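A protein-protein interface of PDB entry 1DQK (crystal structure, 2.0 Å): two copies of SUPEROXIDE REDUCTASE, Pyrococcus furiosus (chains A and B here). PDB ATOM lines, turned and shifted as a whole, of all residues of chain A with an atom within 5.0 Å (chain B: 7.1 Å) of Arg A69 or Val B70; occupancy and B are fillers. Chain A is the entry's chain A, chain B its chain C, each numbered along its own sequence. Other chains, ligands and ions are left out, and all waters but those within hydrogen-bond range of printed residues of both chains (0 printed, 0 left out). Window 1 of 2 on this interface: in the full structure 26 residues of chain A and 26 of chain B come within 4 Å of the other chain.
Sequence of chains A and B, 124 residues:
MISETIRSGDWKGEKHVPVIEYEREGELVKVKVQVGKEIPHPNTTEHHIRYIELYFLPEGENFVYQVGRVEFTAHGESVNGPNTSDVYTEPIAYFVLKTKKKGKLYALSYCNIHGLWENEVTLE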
ATOM      1  N   TYR A  51       2.564  37.806 -24.099  1.00  0.00           N
ATOM      2  CA  TYR A  51       2.739  36.475 -24.655  1.00  0.00           C
ATOM      3  C   TYR A  51       1.640  36.064 -25.624  1.00  0.00           C
ATOM      4  O   TYR A  51       0.605  36.728 -25.738  1.00  0.00           O
ATOM      5  CB  TYR A  51       2.785  35.464 -23.510  1.00  0.00           C
ATOM      6  CG  TYR A  51       1.472  35.340 -22.766  1.00  0.00           C
ATOM      7  CD1 TYR A  51       0.405  34.623 -23.311  1.00  0.00           C
ATOM      8  CD2 TYR A  51       1.294  35.935 -21.514  1.00  0.00           C
ATOM      9  CE1 TYR A  51      -0.803  34.498 -22.630  1.00  0.00           C
ATOM     10  CE2 TYR A  51       0.091  35.816 -20.825  1.00  0.00           C
ATOM     11  CZ  TYR A  51      -0.954  35.094 -21.390  1.00  0.00           C
ATOM     12  OH  TYR A  51      -2.146  34.960 -20.714  1.00  0.00           O
ATOM     13  N   ILE A  52       1.880  34.960 -26.320  1.00  0.00           N
ATOM     14  CA  ILE A  52       0.909  34.394 -27.244  1.00  0.00           C
ATOM     15  C   ILE A  52       0.929  32.890 -26.988  1.00  0.00           C
ATOM     16  O   ILE A  52       1.996  32.291 -26.828  1.00  0.00           O
ATOM     17  CB  ILE A  52       1.283  34.636 -28.727  1.00  0.00           C
ATOM     18  CG1 ILE A  52       0.913  36.058 -29.150  1.00  0.00           C
ATOM     19  CG2 ILE A  52       0.543  33.635 -29.619  1.00  0.00           C
ATOM     20  CD1 ILE A  52       1.442  36.416 -30.537  1.00  0.00           C
ATOM     21  N   GLU A  53      -0.252  32.287 -26.939  1.00  0.00           N
ATOM     22  CA  GLU A  53      -0.369  30.854 -26.723  1.00  0.00           C
ATOM     23  C   GLU A  53      -1.138  30.265 -27.896  1.00  0.00           C
ATOM     24  O   GLU A  53      -2.070  30.892 -28.424  1.00  0.00           O
ATOM     25  CB  GLU A  53      -1.130  30.563 -25.427  1.00  0.00           C
ATOM     26  CG  GLU A  53      -0.390  30.907 -24.157  1.00  0.00           C
ATOM     27  CD  GLU A  53      -1.272  30.761 -22.924  1.00  0.00           C
ATOM     28  OE1 GLU A  53      -2.515  30.718 -23.070  1.00  0.00           O
ATOM     29  OE2 GLU A  53      -0.723  30.688 -21.806  1.00  0.00           O
ATOM     30  N   VAL A  67      -0.524  23.770 -27.715  1.00  0.00           N
ATOM     31  CA  VAL A  67       0.591  23.433 -28.583  1.00  0.00           C
ATOM     32  C   VAL A  67       1.863  24.112 -28.095  1.00  0.00           C
ATOM     33  O   VAL A  67       2.948  23.528 -28.146  1.00  0.00           O
ATOM     34  CB  VAL A  67       0.305  23.857 -30.048  1.00  0.00           C
ATOM     35  CG1 VAL A  67       1.569  23.734 -30.898  1.00  0.00           C
ATOM     36  CG2 VAL A  67      -0.789  22.985 -30.617  1.00  0.00           C
ATOM     37  N   GLY A  68       1.730  25.341 -27.612  1.00  0.00           N
ATOM     38  CA  GLY A  68       2.902  26.039 -27.130  1.00  0.00           C
ATOM     39  C   GLY A  68       2.607  27.411 -26.571  1.00  0.00           C
ATOM     40  O   GLY A  68       1.484  27.919 -26.669  1.00  0.00           O
ATOM     41  N   ARG A  69       3.636  28.016 -25.990  1.00  0.00           N
ATOM     42  CA  ARG A  69       3.505  29.329 -25.395  1.00  0.00           C
ATOM     43  C   ARG A  69       4.783  30.126 -25.605  1.00  0.00           C
ATOM     44  O   ARG A  69       5.890  29.624 -25.365  1.00  0.00           O
ATOM     45  CB  ARG A  69       3.199  29.164 -23.902  1.00  0.00           C
ATOM     46  CG  ARG A  69       3.363  30.404 -23.070  1.00  0.00           C
ATOM     47  CD  ARG A  69       3.017  30.118 -21.599  1.00  0.00           C
ATOM     48  NE  ARG A  69       3.563  31.167 -20.751  1.00  0.00           N
ATOM     49  CZ  ARG A  69       2.855  32.192 -20.291  1.00  0.00           C
ATOM     50  NH1 ARG A  69       1.570  32.307 -20.594  1.00  0.00           N
ATOM     51  NH2 ARG A  69       3.450  33.136 -19.582  1.00  0.00           N
ATOM     52  N   VAL A  70       4.633  31.362 -26.066  1.00  0.00           N
ATOM     53  CA  VAL A  70       5.782  32.222 -26.293  1.00  0.00           C
ATOM     54  C   VAL A  70       5.639  33.490 -25.467  1.00  0.00           C
ATOM     55  O   VAL A  70       4.643  34.217 -25.592  1.00  0.00           O
ATOM     56  CB  VAL A  70       5.920  32.643 -27.783  1.00  0.00           C
ATOM     57  CG1 VAL A  70       7.177  33.512 -27.955  1.00  0.00           C
ATOM     58  CG2 VAL A  70       6.000  31.418 -28.673  1.00  0.00           C
ATOM     59  N   GLU A  71       6.635  33.748 -24.623  1.00  0.00           N
ATOM     60  CA  GLU A  71       6.642  34.939 -23.785  1.00  0.00           C
ATOM     61  C   GLU A  71       7.633  35.943 -24.361  1.00  0.00           C
ATOM     62  O   GLU A  71       8.779  35.602 -24.634  1.00  0.00           O
ATOM     63  CB  GLU A  71       7.037  34.580 -22.336  1.00  0.00           C
ATOM     64  CG  GLU A  71       6.096  33.566 -21.684  1.00  0.00           C
ATOM     65  CD  GLU A  71       6.512  33.140 -20.276  1.00  0.00           C
ATOM     66  OE1 GLU A  71       5.821  32.274 -19.704  1.00  0.00           O
ATOM     67  OE2 GLU A  71       7.514  33.652 -19.737  1.00  0.00           O
ATOM     68  N   PHE A  95       5.513  28.432 -34.171  1.00  0.00           N
ATOM     69  CA  PHE A  95       5.381  27.110 -33.573  1.00  0.00           C
ATOM     70  C   PHE A  95       5.508  26.045 -34.654  1.00  0.00           C
ATOM     71  O   PHE A  95       4.857  26.129 -35.708  1.00  0.00           O
ATOM     72  CB  PHE A  95       4.014  26.943 -32.896  1.00  0.00           C
ATOM     73  CG  PHE A  95       3.690  27.990 -31.869  1.00  0.00           C
ATOM     74  CD1 PHE A  95       3.018  29.155 -32.232  1.00  0.00           C
ATOM     75  CD2 PHE A  95       4.021  27.797 -30.527  1.00  0.00           C
ATOM     76  CE1 PHE A  95       2.667  30.107 -31.273  1.00  0.00           C
ATOM     77  CE2 PHE A  95       3.674  28.743 -29.555  1.00  0.00           C
ATOM     78  CZ  PHE A  95       2.998  29.900 -29.930  1.00  0.00           C
ATOM     79  N   ILE B  49      11.836  17.843 -24.912  1.00  0.00           N
ATOM     80  CA  ILE B  49      12.385  19.137 -24.531  1.00  0.00           C
ATOM     81  C   ILE B  49      11.181  19.974 -24.107  1.00  0.00           C
ATOM     82  O   ILE B  49      10.196  20.070 -24.844  1.00  0.00           O
ATOM     83  CB  ILE B  49      13.120  19.813 -25.718  1.00  0.00           C
ATOM     84  CG1 ILE B  49      14.289  18.930 -26.173  1.00  0.00           C
ATOM     85  CG2 ILE B  49      13.645  21.199 -25.303  1.00  0.00           C
ATOM     86  CD1 ILE B  49      15.274  18.564 -25.050  1.00  0.00           C
ATOM     87  N   ARG B  50      11.255  20.565 -22.918  1.00  0.00           N
ATOM     88  CA  ARG B  50      10.157  21.359 -22.385  1.00  0.00           C
ATOM     89  C   ARG B  50      10.122  22.800 -22.880  1.00  0.00           C
ATOM     90  O   ARG B  50       9.045  23.335 -23.165  1.00  0.00           O
ATOM     91  CB  ARG B  50      10.209  21.372 -20.845  1.00  0.00           C
ATOM     92  CG  ARG B  50       9.951  20.016 -20.183  1.00  0.00           C
ATOM     93  CD  ARG B  50       8.450  19.765 -20.012  1.00  0.00           C
ATOM     94  NE  ARG B  50       8.172  18.545 -19.254  1.00  0.00           N
ATOM     95  CZ  ARG B  50       8.221  18.463 -17.926  1.00  0.00           C
ATOM     96  NH1 ARG B  50       8.539  19.529 -17.203  1.00  0.00           N
ATOM     97  NH2 ARG B  50       7.960  17.314 -17.317  1.00  0.00           N
ATOM     98  N   TYR B  51      11.286  23.437 -22.976  1.00  0.00           N
ATOM     99  CA  TYR B  51      11.328  24.826 -23.413  1.00  0.00           C
ATOM    100  C   TYR B  51      12.724  25.307 -23.754  1.00  0.00           C
ATOM    101  O   TYR B  51      13.721  24.638 -23.472  1.00  0.00           O
ATOM    102  CB  TYR B  51      10.781  25.726 -22.302  1.00  0.00           C
ATOM    103  CG  TYR B  51      11.643  25.728 -21.046  1.00  0.00           C
ATOM    104  CD1 TYR B  51      12.835  26.453 -20.994  1.00  0.00           C
ATOM    105  CD2 TYR B  51      11.259  25.014 -19.908  1.00  0.00           C
ATOM    106  CE1 TYR B  51      13.629  26.470 -19.840  1.00  0.00           C
ATOM    107  CE2 TYR B  51      12.043  25.019 -18.746  1.00  0.00           C
ATOM    108  CZ  TYR B  51      13.227  25.753 -18.720  1.00  0.00           C
ATOM    109  OH  TYR B  51      14.012  25.772 -17.585  1.00  0.00           O
ATOM    110  N   ILE B  52      12.774  26.491 -24.348  1.00  0.00           N
ATOM    111  CA  ILE B  52      14.023  27.140 -24.695  1.00  0.00           C
ATOM    112  C   ILE B  52      13.862  28.613 -24.318  1.00  0.00           C
ATOM    113  O   ILE B  52      12.844  29.233 -24.638  1.00  0.00           O
ATOM    114  CB  ILE B  52      14.318  27.062 -26.209  1.00  0.00           C
ATOM    115  CG1 ILE B  52      14.778  25.650 -26.587  1.00  0.00           C
ATOM    116  CG2 ILE B  52      15.379  28.099 -26.578  1.00  0.00           C
ATOM    117  CD1 ILE B  52      15.039  25.479 -28.085  1.00  0.00           C
ATOM    118  N   GLU B  53      14.859  29.160 -23.631  1.00  0.00           N
ATOM    119  CA  GLU B  53      14.850  30.560 -23.228  1.00  0.00           C
ATOM    120  C   GLU B  53      16.027  31.243 -23.914  1.00  0.00           C
ATOM    121  O   GLU B  53      17.079  30.624 -24.115  1.00  0.00           O
ATOM    122  CB  GLU B  53      14.999  30.690 -21.702  1.00  0.00           C
ATOM    123  CG  GLU B  53      13.799  30.186 -20.909  1.00  0.00           C
ATOM    124  CD  GLU B  53      14.033  30.156 -19.394  1.00  0.00           C
ATOM    125  OE1 GLU B  53      15.196  30.197 -18.944  1.00  0.00           O
ATOM    126  OE2 GLU B  53      13.039  30.086 -18.644  1.00  0.00           O
ATOM    127  N   LEU B  54      15.849  32.514 -24.272  1.00  0.00           N
ATOM    128  CA  LEU B  54      16.900  33.291 -24.925  1.00  0.00           C
ATOM    129  C   LEU B  54      17.199  34.533 -24.096  1.00  0.00           C
ATOM    130  O   LEU B  54      16.285  35.283 -23.723  1.00  0.00           O
ATOM    131  CB  LEU B  54      16.470  33.708 -26.340  1.00  0.00           C
ATOM    132  CG  LEU B  54      17.489  34.527 -27.155  1.00  0.00           C
ATOM    133  CD1 LEU B  54      18.652  33.634 -27.592  1.00  0.00           C
ATOM    134  CD2 LEU B  54      16.806  35.133 -28.377  1.00  0.00           C
ATOM    135  N   GLY B  68      13.187  36.182 -24.338  1.00  0.00           N
ATOM    136  CA  GLY B  68      11.946  35.457 -24.480  1.00  0.00           C
ATOM    137  C   GLY B  68      12.043  34.026 -24.014  1.00  0.00           C
ATOM    138  O   GLY B  68      13.126  33.531 -23.692  1.00  0.00           O
ATOM    139  N   ARG B  69      10.899  33.359 -23.998  1.00  0.00           N
ATOM    140  CA  ARG B  69      10.828  31.977 -23.569  1.00  0.00           C
ATOM    141  C   ARG B  69       9.765  31.261 -24.399  1.00  0.00           C
ATOM    142  O   ARG B  69       8.654  31.768 -24.576  1.00  0.00           O
ATOM    143  CB  ARG B  69      10.482  31.950 -22.076  1.00  0.00           C
ATOM    144  CG  ARG B  69       9.912  30.659 -21.562  1.00  0.00           C
ATOM    145  CD  ARG B  69       9.560  30.787 -20.077  1.00  0.00           C
ATOM    146  NE  ARG B  69       8.742  29.662 -19.652  1.00  0.00           N
ATOM    147  CZ  ARG B  69       9.225  28.579 -19.055  1.00  0.00           C
ATOM    148  NH1 ARG B  69      10.523  28.479 -18.811  1.00  0.00           N
ATOM    149  NH2 ARG B  69       8.411  27.583 -18.733  1.00  0.00           N
ATOM    150  N   VAL B  70      10.119  30.093 -24.925  1.00  0.00           N
ATOM    151  CA  VAL B  70       9.190  29.307 -25.720  1.00  0.00           C
ATOM    152  C   VAL B  70       8.979  27.940 -25.070  1.00  0.00           C
ATOM    153  O   VAL B  70       9.927  27.182 -24.888  1.00  0.00           O
ATOM    154  CB  VAL B  70       9.720  29.085 -27.155  1.00  0.00           C
ATOM    155  CG1 VAL B  70       8.730  28.227 -27.939  1.00  0.00           C
ATOM    156  CG2 VAL B  70       9.930  30.422 -27.848  1.00  0.00           C
ATOM    157  N   GLU B  71       7.740  27.636 -24.705  1.00  0.00           N
ATOM    158  CA  GLU B  71       7.428  26.345 -24.100  1.00  0.00           C
ATOM    159  C   GLU B  71       6.780  25.448 -25.146  1.00  0.00           C
ATOM    160  O   GLU B  71       5.841  25.864 -25.827  1.00  0.00           O
ATOM    161  CB  GLU B  71       6.470  26.516 -22.911  1.00  0.00           C
ATOM    162  CG  GLU B  71       7.001  27.439 -21.820  1.00  0.00           C
ATOM    163  CD  GLU B  71       5.968  27.747 -20.742  1.00  0.00           C
ATOM    164  OE1 GLU B  71       6.297  28.521 -19.822  1.00  0.00           O
ATOM    165  OE2 GLU B  71       4.837  27.222 -20.809  1.00  0.00           O
ATOM    166  N   PHE B  72       7.315  24.237 -25.285  1.00  0.00           N
ATOM    167  CA  PHE B  72       6.809  23.232 -26.222  1.00  0.00           C
ATOM    168  C   PHE B  72       5.973  22.335 -25.330  1.00  0.00           C
ATOM    169  O   PHE B  72       6.501  21.496 -24.597  1.00  0.00           O
ATOM    170  CB  PHE B  72       7.977  22.464 -26.841  1.00  0.00           C
ATOM    171  CG  PHE B  72       9.109  23.353 -27.284  1.00  0.00           C
ATOM    172  CD1 PHE B  72      10.367  23.241 -26.702  1.00  0.00           C
ATOM    173  CD2 PHE B  72       8.906  24.324 -28.266  1.00  0.00           C
ATOM    174  CE1 PHE B  72      11.415  24.089 -27.087  1.00  0.00           C
ATOM    175  CE2 PHE B  72       9.943  25.176 -28.659  1.00  0.00           C
ATOM    176  CZ  PHE B  72      11.203  25.056 -28.064  1.00  0.00           C
ATOM    177  N   THR B  73       4.661  22.507 -25.418  1.00  0.00           N
ATOM    178  CA  THR B  73       3.731  21.810 -24.547  1.00  0.00           C
ATOM    179  C   THR B  73       2.979  20.558 -24.981  1.00  0.00           C
ATOM    180  O   THR B  73       2.273  19.970 -24.161  1.00  0.00           O
ATOM    181  CB  THR B  73       2.702  22.827 -24.031  1.00  0.00           C
ATOM    182  OG1 THR B  73       1.980  23.371 -25.145  1.00  0.00           O
ATOM    183  CG2 THR B  73       3.420  23.969 -23.300  1.00  0.00           C
ATOM    184  N   THR B  89       4.945  19.070 -30.282  1.00  0.00           N
ATOM    185  CA  THR B  89       5.516  20.392 -30.521  1.00  0.00           C
ATOM    186  C   THR B  89       7.033  20.236 -30.562  1.00  0.00           C
ATOM    187  O   THR B  89       7.662  19.888 -29.560  1.00  0.00           O
ATOM    188  CB  THR B  89       5.145  21.385 -29.399  1.00  0.00           C
ATOM    189  OG1 THR B  89       3.726  21.396 -29.224  1.00  0.00           O
ATOM    190  CG2 THR B  89       5.618  22.804 -29.756  1.00  0.00           C
ATOM    191  N   GLU B  90       7.612  20.490 -31.730  1.00  0.00           N
ATOM    192  CA  GLU B  90       9.044  20.361 -31.924  1.00  0.00           C
ATOM    193  C   GLU B  90       9.814  21.476 -31.220  1.00  0.00           C
ATOM    194  O   GLU B  90       9.367  22.625 -31.174  1.00  0.00           O
ATOM    195  CB  GLU B  90       9.362  20.352 -33.425  1.00  0.00           C
ATOM    196  CG  GLU B  90       8.865  19.105 -34.137  1.00  0.00           C
ATOM    197  CD  GLU B  90       9.451  17.831 -33.551  1.00  0.00           C
ATOM    198  OE1 GLU B  90      10.612  17.506 -33.872  1.00  0.00           O
ATOM    199  OE2 GLU B  90       8.753  17.156 -32.764  1.00  0.00           O
ATOM    200  N   PRO B  91      10.992  21.143 -30.669  1.00  0.00           N
ATOM    201  CA  PRO B  91      11.861  22.081 -29.948  1.00  0.00           C
ATOM    202  C   PRO B  91      12.581  23.091 -30.819  1.00  0.00           C
ATOM    203  O   PRO B  91      13.815  23.151 -30.831  1.00  0.00           O
ATOM    204  CB  PRO B  91      12.836  21.168 -29.216  1.00  0.00           C
ATOM    205  CG  PRO B  91      12.932  19.968 -30.090  1.00  0.00           C
ATOM    206  CD  PRO B  91      11.569  19.787 -30.710  1.00  0.00           C
ATOM    207  N   ILE B  92      11.804  23.889 -31.542  1.00  0.00           N
ATOM    208  CA  ILE B  92      12.358  24.915 -32.417  1.00  0.00           C
ATOM    209  C   ILE B  92      11.741  26.240 -32.003  1.00  0.00           C
ATOM    210  O   ILE B  92      10.521  26.419 -32.098  1.00  0.00           O
ATOM    211  CB  ILE B  92      12.018  24.640 -33.896  1.00  0.00           C
ATOM    212  CG1 ILE B  92      12.591  23.290 -34.320  1.00  0.00           C
ATOM    213  CG2 ILE B  92      12.605  25.733 -34.773  1.00  0.00           C
ATOM    214  CD1 ILE B  92      12.029  22.774 -35.641  1.00  0.00           C
ATOM    215  N   ALA B  93      12.586  27.164 -31.551  1.00  0.00           N
ATOM    216  CA  ALA B  93      12.119  28.468 -31.083  1.00  0.00           C
ATOM    217  C   ALA B  93      12.643  29.641 -31.900  1.00  0.00           C
ATOM    218  O   ALA B  93      13.825  29.699 -32.247  1.00  0.00           O
ATOM    219  CB  ALA B  93      12.503  28.657 -29.615  1.00  0.00           C
ATOM    220  N   TYR B  94      11.752  30.579 -32.191  1.00  0.00           N
ATOM    221  CA  TYR B  94      12.109  31.760 -32.956  1.00  0.00           C
ATOM    222  C   TYR B  94      11.786  33.001 -32.138  1.00  0.00           C
ATOM    223  O   TYR B  94      10.714  33.097 -31.534  1.00  0.00           O
ATOM    224  CB  TYR B  94      11.332  31.806 -34.277  1.00  0.00           C
ATOM    225  CG  TYR B  94      11.255  30.484 -35.005  1.00  0.00           C
ATOM    226  CD1 TYR B  94      10.476  29.437 -34.513  1.00  0.00           C
ATOM    227  CD2 TYR B  94      11.946  30.285 -36.198  1.00  0.00           C
ATOM    228  CE1 TYR B  94      10.384  28.227 -35.192  1.00  0.00           C
ATOM    229  CE2 TYR B  94      11.860  29.078 -36.884  1.00  0.00           C
ATOM    230  CZ  TYR B  94      11.079  28.056 -36.377  1.00  0.00           C
ATOM    231  OH  TYR B  94      10.996  26.862 -37.055  1.00  0.00           O
ATOM    232  N   PHE B  95      12.720  33.943 -32.120  1.00  0.00           N
ATOM    233  CA  PHE B  95      12.546  35.189 -31.386  1.00  0.00           C
ATOM    234  C   PHE B  95      12.867  36.376 -32.288  1.00  0.00           C
ATOM    235  O   PHE B  95      13.901  36.385 -32.965  1.00  0.00           O
ATOM    236  CB  PHE B  95      13.486  35.236 -30.178  1.00  0.00           C
ATOM    237  CG  PHE B  95      13.346  34.069 -29.242  1.00  0.00           C
ATOM    238  CD1 PHE B  95      14.099  32.914 -29.434  1.00  0.00           C
ATOM    239  CD2 PHE B  95      12.488  34.135 -28.150  1.00  0.00           C
ATOM    240  CE1 PHE B  95      14.002  31.841 -28.548  1.00  0.00           C
ATOM    241  CE2 PHE B  95      12.381  33.062 -27.249  1.00  0.00           C
ATOM    242  CZ  PHE B  95      13.140  31.914 -27.450  1.00  0.00           C
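OE1 of Glu A71 is in salt-bridge range of NE of Arg B69, 3.9 Å away.
The guanidinium group of Arg A69 is in salt-bridge range of the side-chain carboxylate of Glu B71.
The backbone carbonyl oxygen (O) of Val A67 sits close to the side-chain hydroxyl (OG1) of Thr B73 (3.2 Å).
The backbone carbonyl oxygen (O) of Val A67 is in hydrogen-bond range of the side-chain hydroxyl (OG1) of Thr B89 (2.5 Å).
OG1 of Thr B73 lies within hydrogen-bond range of N of Gly A68 (3.2 Å).
OE2 of Glu A53 lies within salt-bridge range of NH1 of Arg A69 (3.1 Å).
The side-chain carboxylate (OE1) of Glu B71 lies within salt-bridge range of the guanidinium group (NH2) of Arg B69, 2.6 Å away.
The side-chain carboxylate of Glu B53 lies within salt-bridge range of the guanidinium group of Arg B69 (3.0 Å).
The backbone NH (N) of Val A70 is in hydrogen-bond range of the backbone carbonyl oxygen (O) of Ile A52, at 2.9 Å.
The backbone NH (N) of Leu B54 is in hydrogen-bond range of the backbone carbonyl oxygen (O) of Gly B68 (3.0 Å).
O of Ile B52 lies within hydrogen-bond range of N of Val B70, 2.9 Å away.
Among the printed residues, merely in contact across the chains: Gly A68 with Glu B71 (3.2 Å), Arg A69 with Arg B69 (3.6 Å), Arg A69 with Val B70 (3.3 Å), Val A70 with Arg B69 (3.4 Å), Glu A71 with Gly B68 (3.2 Å) and Glu A71 with Glu B71 (3.8 Å).
Of chain B, only Arg B69 (3.6 Å), Val B70 (3.3 Å) and Glu B71 (2.8 Å) come within 4 Å of Arg A69.
Val B70 touches just one residue of chain A: Arg A69 (3.3 Å).
Of the printed residues of chain A, Glu B71 touches Gly A68, Arg A69 and Glu A71.
Printed residues of chain A within 4 Å of Thr B73: Val A67 (3.0 Å) and Gly A68 (3.2 Å).
Printed residues of chain A within 4 Å of Thr B89: Val A67 (2.5 Å).
Of the printed residues of chain B, Val A67 touches Thr B73 and Thr B89.
Of the printed residues of chain B, Glu A71 touches Gly B68, Arg B69 and Glu B71.
The nearest residue of chain A that does not touch Val B70 is Val A70 (4.1 Å).
Hydrophobic or aromatic side chains of chain A that line the printed part of chain B: Val A67.
Of the 19 printed residues of chain B, 6 touch a printed residue of chain A.
Among the printed residues, Asp or Glu carboxylates within 4 Å of a Lys or Arg side-chain nitrogen of the other chain: Arg A69 with Glu B71 and Glu A71 with Arg B69.
Gly A68 touches Glu B71, and with the chains exchanged Glu A71 touches Gly B68.
Arg A69 touches Val B70, and with the chains exchanged Val A70 touches Arg B69.
Arg A69 touches Glu B71, and with the chains exchanged Glu A71 touches Arg B69.
Glu A71 touches its own counterpart, Glu B71.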
